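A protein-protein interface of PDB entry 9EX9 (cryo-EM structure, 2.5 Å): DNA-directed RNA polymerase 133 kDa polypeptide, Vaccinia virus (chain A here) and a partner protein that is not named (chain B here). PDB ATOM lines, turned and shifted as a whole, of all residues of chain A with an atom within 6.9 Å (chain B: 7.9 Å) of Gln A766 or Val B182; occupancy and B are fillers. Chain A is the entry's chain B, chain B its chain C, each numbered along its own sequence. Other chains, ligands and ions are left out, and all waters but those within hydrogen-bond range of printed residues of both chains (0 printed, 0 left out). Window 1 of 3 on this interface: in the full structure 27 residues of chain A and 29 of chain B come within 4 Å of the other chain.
Hydrophobic or aromatic side chains of chain B that line the printed part of chain A: His B58 and Val B182. Among the printed residues, 5 pairs touch across the chains. Among the printed residues, Asp or Glu carboxylates within 4 Å of a Lys or Arg side-chain nitrogen of the other chain: Arg A876 with Glu B57 (3.5 Å).
O of Gln A763 lies close to NE of Arg A767. The side-chain carboxylate (OD1) of Asp A771 lies within hydrogen-bond range of the backbone NH (N) of Arg A876, at 3.4 Å. N of Leu B34 lies within hydrogen-bond range of O of Val B182 (3.2 Å). The backbone carbonyl oxygen (O) of Glu B57 is in hydrogen-bond range of the backbone NH (N) of Leu B35, at 3.4 Å. The side-chain hydroxyl (OG) of Ser B146 sits at hydrogen-bond distance from the backbone NH (N) of Val B182.
Of the printed residues of chain B, Arg A876 touches Thr B54 (3.7 Å) and Glu B57 (3.5 Å). Of the printed residues of chain A, Glu B57 touches Arg A876 (3.5 Å). Of the printed residues of chain A, His B58 touches Gln A766 and Arg A767. The nearest printed residue of chain B that does not touch Gln A766 is Thr B54 (4.5 Å).
O of Gln A766 is in hydrogen-bond range of NE2 of His B58, at 2.8 Å. The guanidinium group of Arg A876 is in salt-bridge range of the side-chain carboxylate of Glu B57.
Among the printed residues, merely in contact across the chains: Arg A767 with His B58 (3.4 Å), Arg A876 with Thr B54 (3.7 Å) and Gln A766 with Val B182 (3.9997 Å).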
ATOM      1  N   LYS A 761      -5.135  21.389 -14.268  1.00  0.00           N
ATOM      2  CA  LYS A 761      -4.026  20.699 -14.908  1.00  0.00           C
ATOM      3  C   LYS A 761      -3.124  20.046 -13.874  1.00  0.00           C
ATOM      4  O   LYS A 761      -2.865  20.611 -12.811  1.00  0.00           O
ATOM      5  CB  LYS A 761      -3.215  21.673 -15.758  1.00  0.00           C
ATOM      6  CG  LYS A 761      -2.041  21.044 -16.460  1.00  0.00           C
ATOM      7  CD  LYS A 761      -1.509  21.927 -17.567  1.00  0.00           C
ATOM      8  CE  LYS A 761      -0.983  23.237 -17.045  1.00  0.00           C
ATOM      9  NZ  LYS A 761      -0.354  24.038 -18.122  1.00  0.00           N
ATOM     10  N   LYS A 762      -2.635  18.852 -14.203  1.00  0.00           N
ATOM     11  CA  LYS A 762      -1.882  18.062 -13.237  1.00  0.00           C
ATOM     12  C   LYS A 762      -0.489  18.634 -12.998  1.00  0.00           C
ATOM     13  O   LYS A 762      -0.030  18.699 -11.854  1.00  0.00           O
ATOM     14  CB  LYS A 762      -1.793  16.618 -13.721  1.00  0.00           C
ATOM     15  CG  LYS A 762      -1.012  15.702 -12.819  1.00  0.00           C
ATOM     16  CD  LYS A 762      -0.803  14.357 -13.467  1.00  0.00           C
ATOM     17  CE  LYS A 762       0.204  13.536 -12.694  1.00  0.00           C
ATOM     18  NZ  LYS A 762       0.493  12.241 -13.359  1.00  0.00           N
ATOM     19  N   GLN A 763       0.208  19.032 -14.060  1.00  0.00           N
ATOM     20  CA  GLN A 763       1.554  19.566 -13.888  1.00  0.00           C
ATOM     21  C   GLN A 763       1.539  20.900 -13.157  1.00  0.00           C
ATOM     22  O   GLN A 763       2.522  21.255 -12.502  1.00  0.00           O
ATOM     23  CB  GLN A 763       2.240  19.716 -15.243  1.00  0.00           C
ATOM     24  CG  GLN A 763       2.748  18.419 -15.829  1.00  0.00           C
ATOM     25  CD  GLN A 763       1.640  17.449 -16.143  1.00  0.00           C
ATOM     26  OE1 GLN A 763       0.480  17.700 -15.836  1.00  0.00           O
ATOM     27  NE2 GLN A 763       1.989  16.332 -16.753  1.00  0.00           N
ATOM     28  N   PHE A 764       0.447  21.653 -13.272  1.00  0.00           N
ATOM     29  CA  PHE A 764       0.305  22.888 -12.509  1.00  0.00           C
ATOM     30  C   PHE A 764       0.222  22.603 -11.015  1.00  0.00           C
ATOM     31  O   PHE A 764       0.794  23.336 -10.204  1.00  0.00           O
ATOM     32  CB  PHE A 764      -0.935  23.638 -12.994  1.00  0.00           C
ATOM     33  CG  PHE A 764      -1.307  24.825 -12.161  1.00  0.00           C
ATOM     34  CD1 PHE A 764      -0.587  25.999 -12.242  1.00  0.00           C
ATOM     35  CD2 PHE A 764      -2.399  24.777 -11.317  1.00  0.00           C
ATOM     36  CE1 PHE A 764      -0.938  27.091 -11.490  1.00  0.00           C
ATOM     37  CE2 PHE A 764      -2.748  25.868 -10.562  1.00  0.00           C
ATOM     38  CZ  PHE A 764      -2.015  27.027 -10.650  1.00  0.00           C
ATOM     39  N   ILE A 765      -0.489  21.541 -10.635  1.00  0.00           N
ATOM     40  CA  ILE A 765      -0.584  21.162  -9.229  1.00  0.00           C
ATOM     41  C   ILE A 765       0.742  20.612  -8.728  1.00  0.00           C
ATOM     42  O   ILE A 765       1.167  20.906  -7.608  1.00  0.00           O
ATOM     43  CB  ILE A 765      -1.718  20.145  -9.029  1.00  0.00           C
ATOM     44  CG1 ILE A 765      -3.069  20.811  -9.264  1.00  0.00           C
ATOM     45  CG2 ILE A 765      -1.642  19.547  -7.644  1.00  0.00           C
ATOM     46  CD1 ILE A 765      -4.200  19.843  -9.409  1.00  0.00           C
ATOM     47  N   GLN A 766       1.412  19.796  -9.541  1.00  0.00           N
ATOM     48  CA  GLN A 766       2.687  19.229  -9.119  1.00  0.00           C
ATOM     49  C   GLN A 766       3.721  20.312  -8.861  1.00  0.00           C
ATOM     50  O   GLN A 766       4.517  20.207  -7.923  1.00  0.00           O
ATOM     51  CB  GLN A 766       3.210  18.257 -10.170  1.00  0.00           C
ATOM     52  CG  GLN A 766       2.546  16.905 -10.163  1.00  0.00           C
ATOM     53  CD  GLN A 766       3.101  15.994 -11.233  1.00  0.00           C
ATOM     54  OE1 GLN A 766       3.633  16.453 -12.238  1.00  0.00           O
ATOM     55  NE2 GLN A 766       2.985  14.694 -11.020  1.00  0.00           N
ATOM     56  N   ARG A 767       3.747  21.350  -9.690  1.00  0.00           N
ATOM     57  CA  ARG A 767       4.784  22.364  -9.577  1.00  0.00           C
ATOM     58  C   ARG A 767       4.563  23.312  -8.409  1.00  0.00           C
ATOM     59  O   ARG A 767       5.496  24.029  -8.037  1.00  0.00           O
ATOM     60  CB  ARG A 767       4.882  23.143 -10.885  1.00  0.00           C
ATOM     61  CG  ARG A 767       5.471  22.317 -12.013  1.00  0.00           C
ATOM     62  CD  ARG A 767       5.756  23.143 -13.247  1.00  0.00           C
ATOM     63  NE  ARG A 767       4.661  23.127 -14.211  1.00  0.00           N
ATOM     64  CZ  ARG A 767       4.680  22.500 -15.381  1.00  0.00           C
ATOM     65  NH1 ARG A 767       5.729  21.807 -15.783  1.00  0.00           N
ATOM     66  NH2 ARG A 767       3.617  22.576 -16.172  1.00  0.00           N
ATOM     67  N   GLY A 768       3.377  23.324  -7.813  1.00  0.00           N
ATOM     68  CA  GLY A 768       3.134  24.136  -6.640  1.00  0.00           C
ATOM     69  C   GLY A 768       1.990  25.111  -6.801  1.00  0.00           C
ATOM     70  O   GLY A 768       1.862  26.049  -6.013  1.00  0.00           O
ATOM     71  N   GLY A 769       1.147  24.909  -7.803  1.00  0.00           N
ATOM     72  CA  GLY A 769       0.090  25.855  -8.089  1.00  0.00           C
ATOM     73  C   GLY A 769      -0.984  25.942  -7.028  1.00  0.00           C
ATOM     74  O   GLY A 769      -1.694  24.971  -6.774  1.00  0.00           O
ATOM     75  N   ASP A 771      -0.787  26.063  -3.866  1.00  0.00           N
ATOM     76  CA  ASP A 771      -0.516  25.151  -2.767  1.00  0.00           C
ATOM     77  C   ASP A 771      -0.633  25.887  -1.438  1.00  0.00           C
ATOM     78  O   ASP A 771      -0.155  27.015  -1.300  1.00  0.00           O
ATOM     79  CB  ASP A 771       0.885  24.563  -2.928  1.00  0.00           C
ATOM     80  CG  ASP A 771       1.020  23.195  -2.319  1.00  0.00           C
ATOM     81  OD1 ASP A 771       0.021  22.673  -1.791  1.00  0.00           O
ATOM     82  OD2 ASP A 771       2.132  22.638  -2.371  1.00  0.00           O
ATOM     83  N   ARG A 876      -2.147  20.069  -1.570  1.00  0.00           N
ATOM     84  CA  ARG A 876      -2.298  20.362  -2.980  1.00  0.00           C
ATOM     85  C   ARG A 876      -3.754  20.145  -3.391  1.00  0.00           C
ATOM     86  O   ARG A 876      -4.460  19.339  -2.781  1.00  0.00           O
ATOM     87  CB  ARG A 876      -1.380  19.475  -3.808  1.00  0.00           C
ATOM     88  CG  ARG A 876       0.053  19.497  -3.336  1.00  0.00           C
ATOM     89  CD  ARG A 876       0.958  18.727  -4.255  1.00  0.00           C
ATOM     90  NE  ARG A 876       2.359  18.931  -3.922  1.00  0.00           N
ATOM     91  CZ  ARG A 876       3.370  18.363  -4.562  1.00  0.00           C
ATOM     92  NH1 ARG A 876       3.171  17.541  -5.576  1.00  0.00           N
ATOM     93  NH2 ARG A 876       4.613  18.627  -4.175  1.00  0.00           N
ATOM     94  N   ASP A 898      -4.480  15.669 -17.494  1.00  0.00           N
ATOM     95  CA  ASP A 898      -3.055  15.678 -17.761  1.00  0.00           C
ATOM     96  C   ASP A 898      -2.720  16.734 -18.807  1.00  0.00           C
ATOM     97  O   ASP A 898      -3.554  17.139 -19.615  1.00  0.00           O
ATOM     98  CB  ASP A 898      -2.589  14.304 -18.232  1.00  0.00           C
ATOM     99  CG  ASP A 898      -1.094  14.132 -18.119  1.00  0.00           C
ATOM    100  OD1 ASP A 898      -0.601  13.989 -16.985  1.00  0.00           O
ATOM    101  OD2 ASP A 898      -0.409  14.142 -19.159  1.00  0.00           O
ATOM    102  N   LYS B  31      10.823  10.394 -20.403  1.00  0.00           N
ATOM    103  CA  LYS B  31      10.478  10.787 -19.041  1.00  0.00           C
ATOM    104  C   LYS B  31      11.748  11.137 -18.286  1.00  0.00           C
ATOM    105  O   LYS B  31      12.646  10.299 -18.157  1.00  0.00           O
ATOM    106  CB  LYS B  31       9.728   9.665 -18.325  1.00  0.00           C
ATOM    107  CG  LYS B  31       8.470   9.238 -19.033  1.00  0.00           C
ATOM    108  CD  LYS B  31       7.802   8.081 -18.338  1.00  0.00           C
ATOM    109  CE  LYS B  31       6.484   7.754 -18.999  1.00  0.00           C
ATOM    110  NZ  LYS B  31       5.768   6.652 -18.320  1.00  0.00           N
ATOM    111  N   TRP B  32      11.821  12.369 -17.786  1.00  0.00           N
ATOM    112  CA  TRP B  32      12.936  12.802 -16.963  1.00  0.00           C
ATOM    113  C   TRP B  32      12.517  12.769 -15.503  1.00  0.00           C
ATOM    114  O   TRP B  32      11.520  13.414 -15.149  1.00  0.00           O
ATOM    115  CB  TRP B  32      13.376  14.203 -17.357  1.00  0.00           C
ATOM    116  CG  TRP B  32      14.669  14.589 -16.751  1.00  0.00           C
ATOM    117  CD1 TRP B  32      14.854  15.373 -15.664  1.00  0.00           C
ATOM    118  CD2 TRP B  32      15.969  14.192 -17.188  1.00  0.00           C
ATOM    119  NE1 TRP B  32      16.191  15.497 -15.392  1.00  0.00           N
ATOM    120  CE2 TRP B  32      16.896  14.779 -16.318  1.00  0.00           C
ATOM    121  CE3 TRP B  32      16.436  13.395 -18.232  1.00  0.00           C
ATOM    122  CZ2 TRP B  32      18.264  14.597 -16.459  1.00  0.00           C
ATOM    123  CZ3 TRP B  32      17.791  13.219 -18.371  1.00  0.00           C
ATOM    124  CH2 TRP B  32      18.690  13.814 -17.492  1.00  0.00           C
ATOM    125  N   PRO B  33      13.210  12.042 -14.630  1.00  0.00           N
ATOM    126  CA  PRO B  33      12.725  11.890 -13.254  1.00  0.00           C
ATOM    127  C   PRO B  33      12.890  13.155 -12.422  1.00  0.00           C
ATOM    128  O   PRO B  33      13.864  13.897 -12.556  1.00  0.00           O
ATOM    129  CB  PRO B  33      13.589  10.752 -12.709  1.00  0.00           C
ATOM    130  CG  PRO B  33      14.847  10.857 -13.476  1.00  0.00           C
ATOM    131  CD  PRO B  33      14.469  11.312 -14.847  1.00  0.00           C
ATOM    132  N   LEU B  34      11.925  13.385 -11.539  1.00  0.00           N
ATOM    133  CA  LEU B  34      11.951  14.503 -10.610  1.00  0.00           C
ATOM    134  C   LEU B  34      12.612  14.100  -9.297  1.00  0.00           C
ATOM    135  O   LEU B  34      12.640  12.928  -8.920  1.00  0.00           O
ATOM    136  CB  LEU B  34      10.537  15.009 -10.327  1.00  0.00           C
ATOM    137  CG  LEU B  34       9.740  15.599 -11.486  1.00  0.00           C
ATOM    138  CD1 LEU B  34       8.368  16.007 -11.009  1.00  0.00           C
ATOM    139  CD2 LEU B  34      10.455  16.784 -12.090  1.00  0.00           C
ATOM    140  N   LEU B  35      13.136  15.101  -8.590  1.00  0.00           N
ATOM    141  CA  LEU B  35      13.755  14.902  -7.277  1.00  0.00           C
ATOM    142  C   LEU B  35      12.682  14.938  -6.192  1.00  0.00           C
ATOM    143  O   LEU B  35      12.607  15.853  -5.377  1.00  0.00           O
ATOM    144  CB  LEU B  35      14.811  15.966  -7.021  1.00  0.00           C
ATOM    145  CG  LEU B  35      16.096  15.902  -7.833  1.00  0.00           C
ATOM    146  CD1 LEU B  35      16.832  17.212  -7.708  1.00  0.00           C
ATOM    147  CD2 LEU B  35      16.970  14.760  -7.365  1.00  0.00           C
ATOM    148  N   ASN B  36      11.841  13.909  -6.188  1.00  0.00           N
ATOM    149  CA  ASN B  36      10.682  13.888  -5.311  1.00  0.00           C
ATOM    150  C   ASN B  36      10.883  13.058  -4.054  1.00  0.00           C
ATOM    151  O   ASN B  36       9.950  12.956  -3.253  1.00  0.00           O
ATOM    152  CB  ASN B  36       9.456  13.374  -6.066  1.00  0.00           C
ATOM    153  CG  ASN B  36       9.406  11.872  -6.145  1.00  0.00           C
ATOM    154  OD1 ASN B  36      10.164  11.257  -6.886  1.00  0.00           O
ATOM    155  ND2 ASN B  36       8.494  11.272  -5.400  1.00  0.00           N
ATOM    156  N   ILE B  37      12.052  12.461  -3.847  1.00  0.00           N
ATOM    157  CA  ILE B  37      12.327  11.725  -2.613  1.00  0.00           C
ATOM    158  C   ILE B  37      13.169  12.653  -1.747  1.00  0.00           C
ATOM    159  O   ILE B  37      14.392  12.634  -1.800  1.00  0.00           O
ATOM    160  CB  ILE B  37      13.020  10.394  -2.887  1.00  0.00           C
ATOM    161  CG1 ILE B  37      12.146   9.521  -3.786  1.00  0.00           C
ATOM    162  CG2 ILE B  37      13.314   9.672  -1.589  1.00  0.00           C
ATOM    163  CD1 ILE B  37      12.844   8.302  -4.298  1.00  0.00           C
ATOM    164  N   THR B  54       9.009  21.204  -1.915  1.00  0.00           N
ATOM    165  CA  THR B  54       8.332  21.409  -3.189  1.00  0.00           C
ATOM    166  C   THR B  54       9.166  22.271  -4.123  1.00  0.00           C
ATOM    167  O   THR B  54       9.144  22.066  -5.339  1.00  0.00           O
ATOM    168  CB  THR B  54       6.961  22.037  -2.973  1.00  0.00           C
ATOM    169  OG1 THR B  54       6.184  21.208  -2.106  1.00  0.00           O
ATOM    170  CG2 THR B  54       6.239  22.180  -4.293  1.00  0.00           C
ATOM    171  N   ALA B  55       9.901  23.248  -3.587  1.00  0.00           N
ATOM    172  CA  ALA B  55      10.761  24.053  -4.447  1.00  0.00           C
ATOM    173  C   ALA B  55      11.894  23.221  -5.032  1.00  0.00           C
ATOM    174  O   ALA B  55      12.238  23.372  -6.209  1.00  0.00           O
ATOM    175  CB  ALA B  55      11.314  25.240  -3.666  1.00  0.00           C
ATOM    176  N   GLU B  57      11.923  19.961  -5.513  1.00  0.00           N
ATOM    177  CA  GLU B  57      11.477  18.849  -6.343  1.00  0.00           C
ATOM    178  C   GLU B  57      11.585  19.165  -7.830  1.00  0.00           C
ATOM    179  O   GLU B  57      11.745  18.251  -8.644  1.00  0.00           O
ATOM    180  CB  GLU B  57      10.041  18.484  -5.984  1.00  0.00           C
ATOM    181  CG  GLU B  57       9.468  17.341  -6.788  1.00  0.00           C
ATOM    182  CD  GLU B  57       8.073  16.967  -6.344  1.00  0.00           C
ATOM    183  OE1 GLU B  57       7.714  17.266  -5.189  1.00  0.00           O
ATOM    184  OE2 GLU B  57       7.331  16.376  -7.151  1.00  0.00           O
ATOM    185  N   HIS B  58      11.504  20.436  -8.209  1.00  0.00           N
ATOM    186  CA  HIS B  58      11.463  20.835  -9.609  1.00  0.00           C
ATOM    187  C   HIS B  58      12.705  21.620 -10.000  1.00  0.00           C
ATOM    188  O   HIS B  58      12.636  22.590 -10.749  1.00  0.00           O
ATOM    189  CB  HIS B  58      10.202  21.642  -9.902  1.00  0.00           C
ATOM    190  CG  HIS B  58       8.940  20.861  -9.723  1.00  0.00           C
ATOM    191  ND1 HIS B  58       8.405  20.075 -10.719  1.00  0.00           N
ATOM    192  CD2 HIS B  58       8.116  20.731  -8.659  1.00  0.00           C
ATOM    193  CE1 HIS B  58       7.304  19.497 -10.276  1.00  0.00           C
ATOM    194  NE2 HIS B  58       7.106  19.878  -9.029  1.00  0.00           N
ATOM    195  N   ARG B  75      16.700   4.420 -17.311  1.00  0.00           N
ATOM    196  CA  ARG B  75      16.559   4.112 -15.889  1.00  0.00           C
ATOM    197  C   ARG B  75      17.593   3.100 -15.413  1.00  0.00           C
ATOM    198  O   ARG B  75      17.316   2.290 -14.529  1.00  0.00           O
ATOM    199  CB  ARG B  75      15.144   3.633 -15.562  1.00  0.00           C
ATOM    200  CG  ARG B  75      14.091   4.658 -15.917  1.00  0.00           C
ATOM    201  CD  ARG B  75      12.700   4.225 -15.531  1.00  0.00           C
ATOM    202  NE  ARG B  75      12.548   4.109 -14.088  1.00  0.00           N
ATOM    203  CZ  ARG B  75      11.393   3.901 -13.475  1.00  0.00           C
ATOM    204  NH1 ARG B  75      10.260   3.804 -14.151  1.00  0.00           N
ATOM    205  NH2 ARG B  75      11.372   3.788 -12.150  1.00  0.00           N
ATOM    206  N   SER B 145      16.141  11.166  -6.893  1.00  0.00           N
ATOM    207  CA  SER B 145      15.248  11.101  -8.039  1.00  0.00           C
ATOM    208  C   SER B 145      14.169  10.044  -7.823  1.00  0.00           C
ATOM    209  O   SER B 145      14.177   9.290  -6.850  1.00  0.00           O
ATOM    210  CB  SER B 145      16.035  10.803  -9.308  1.00  0.00           C
ATOM    211  OG  SER B 145      16.929   9.727  -9.111  1.00  0.00           O
ATOM    212  N   SER B 146      13.231   9.986  -8.765  1.00  0.00           N
ATOM    213  CA  SER B 146      11.965   9.316  -8.498  1.00  0.00           C
ATOM    214  C   SER B 146      12.126   7.804  -8.377  1.00  0.00           C
ATOM    215  O   SER B 146      11.418   7.165  -7.590  1.00  0.00           O
ATOM    216  CB  SER B 146      10.957   9.664  -9.588  1.00  0.00           C
ATOM    217  OG  SER B 146       9.639   9.376  -9.169  1.00  0.00           O
ATOM    218  N   GLY B 147      13.032   7.208  -9.137  1.00  0.00           N
ATOM    219  CA  GLY B 147      13.098   5.761  -9.154  1.00  0.00           C
ATOM    220  C   GLY B 147      13.926   5.103  -8.073  1.00  0.00           C
ATOM    221  O   GLY B 147      13.932   3.875  -7.981  1.00  0.00           O
ATOM    222  N   ASP B 178       5.164   9.570  -2.112  1.00  0.00           N
ATOM    223  CA  ASP B 178       4.281   8.779  -2.951  1.00  0.00           C
ATOM    224  C   ASP B 178       5.061   7.650  -3.624  1.00  0.00           C
ATOM    225  O   ASP B 178       6.234   7.811  -3.966  1.00  0.00           O
ATOM    226  CB  ASP B 178       3.612   9.650  -4.004  1.00  0.00           C
ATOM    227  CG  ASP B 178       4.599  10.269  -4.953  1.00  0.00           C
ATOM    228  OD1 ASP B 178       5.767  10.450  -4.557  1.00  0.00           O
ATOM    229  OD2 ASP B 178       4.204  10.576  -6.096  1.00  0.00           O
ATOM    230  N   PRO B 179       4.422   6.496  -3.839  1.00  0.00           N
ATOM    231  CA  PRO B 179       5.175   5.317  -4.286  1.00  0.00           C
ATOM    232  C   PRO B 179       5.468   5.273  -5.774  1.00  0.00           C
ATOM    233  O   PRO B 179       6.450   4.628  -6.166  1.00  0.00           O
ATOM    234  CB  PRO B 179       4.258   4.158  -3.887  1.00  0.00           C
ATOM    235  CG  PRO B 179       2.889   4.735  -3.985  1.00  0.00           C
ATOM    236  CD  PRO B 179       3.002   6.184  -3.601  1.00  0.00           C
ATOM    237  N   ASP B 180       4.669   5.924  -6.612  1.00  0.00           N
ATOM    238  CA  ASP B 180       4.782   5.730  -8.049  1.00  0.00           C
ATOM    239  C   ASP B 180       5.803   6.690  -8.657  1.00  0.00           C
ATOM    240  O   ASP B 180       6.344   7.577  -7.994  1.00  0.00           O
ATOM    241  CB  ASP B 180       3.421   5.899  -8.718  1.00  0.00           C
ATOM    242  CG  ASP B 180       2.680   7.109  -8.223  1.00  0.00           C
ATOM    243  OD1 ASP B 180       3.259   7.861  -7.416  1.00  0.00           O
ATOM    244  OD2 ASP B 180       1.518   7.306  -8.634  1.00  0.00           O
ATOM    245  N   PHE B 181       6.070   6.485  -9.944  1.00  0.00           N
ATOM    246  CA  PHE B 181       7.091   7.238 -10.657  1.00  0.00           C
ATOM    247  C   PHE B 181       6.591   8.636 -10.993  1.00  0.00           C
ATOM    248  O   PHE B 181       5.434   8.821 -11.377  1.00  0.00           O
ATOM    249  CB  PHE B 181       7.480   6.491 -11.933  1.00  0.00           C
ATOM    250  CG  PHE B 181       8.704   7.021 -12.610  1.00  0.00           C
ATOM    251  CD1 PHE B 181       9.925   7.002 -11.974  1.00  0.00           C
ATOM    252  CD2 PHE B 181       8.641   7.506 -13.899  1.00  0.00           C
ATOM    253  CE1 PHE B 181      11.051   7.481 -12.603  1.00  0.00           C
ATOM    254  CE2 PHE B 181       9.765   7.982 -14.528  1.00  0.00           C
ATOM    255  CZ  PHE B 181      10.968   7.967 -13.881  1.00  0.00           C
ATOM    256  N   VAL B 182       7.471   9.623 -10.836  1.00  0.00           N
ATOM    257  CA  VAL B 182       7.154  11.024 -11.089  1.00  0.00           C
ATOM    258  C   VAL B 182       8.240  11.600 -11.984  1.00  0.00           C
ATOM    259  O   VAL B 182       9.430  11.438 -11.700  1.00  0.00           O
ATOM    260  CB  VAL B 182       7.044  11.825  -9.781  1.00  0.00           C
ATOM    261  CG1 VAL B 182       6.583  13.233 -10.062  1.00  0.00           C
ATOM    262  CG2 VAL B 182       6.090  11.139  -8.828  1.00  0.00           C
ATOM    263  N   PHE B 183       7.833  12.290 -13.046  1.00  0.00           N
ATOM    264  CA  PHE B 183       8.747  12.679 -14.111  1.00  0.00           C
ATOM    265  C   PHE B 183       8.297  14.004 -14.711  1.00  0.00           C
ATOM    266  O   PHE B 183       7.285  14.581 -14.312  1.00  0.00           O
ATOM    267  CB  PHE B 183       8.795  11.596 -15.186  1.00  0.00           C
ATOM    268  CG  PHE B 183       7.452  11.284 -15.766  1.00  0.00           C
ATOM    269  CD1 PHE B 183       6.638  10.335 -15.185  1.00  0.00           C
ATOM    270  CD2 PHE B 183       6.993  11.960 -16.879  1.00  0.00           C
ATOM    271  CE1 PHE B 183       5.403  10.060 -15.708  1.00  0.00           C
ATOM    272  CE2 PHE B 183       5.757  11.686 -17.403  1.00  0.00           C
ATOM    273  CZ  PHE B 183       4.963  10.736 -16.817  1.00  0.00           C
ATOM    274  N   ARG B 184       9.062  14.479 -15.690  1.00  0.00           N
ATOM    275  CA  ARG B 184       8.709  15.662 -16.457  1.00  0.00           C
ATOM    276  C   ARG B 184       9.146  15.464 -17.898  1.00  0.00           C
ATOM    277  O   ARG B 184      10.003  14.632 -18.199  1.00  0.00           O
ATOM    278  CB  ARG B 184       9.356  16.928 -15.891  1.00  0.00           C
ATOM    279  CG  ARG B 184      10.871  16.908 -15.912  1.00  0.00           C
ATOM    280  CD  ARG B 184      11.449  18.303 -15.900  1.00  0.00           C
ATOM    281  NE  ARG B 184      11.078  19.058 -17.088  1.00  0.00           N
ATOM    282  CZ  ARG B 184      11.473  20.296 -17.342  1.00  0.00           C
ATOM    283  NH1 ARG B 184      12.271  20.951 -16.516  1.00  0.00           N
ATOM    284  NH2 ARG B 184      11.059  20.894 -18.452  1.00  0.00           N
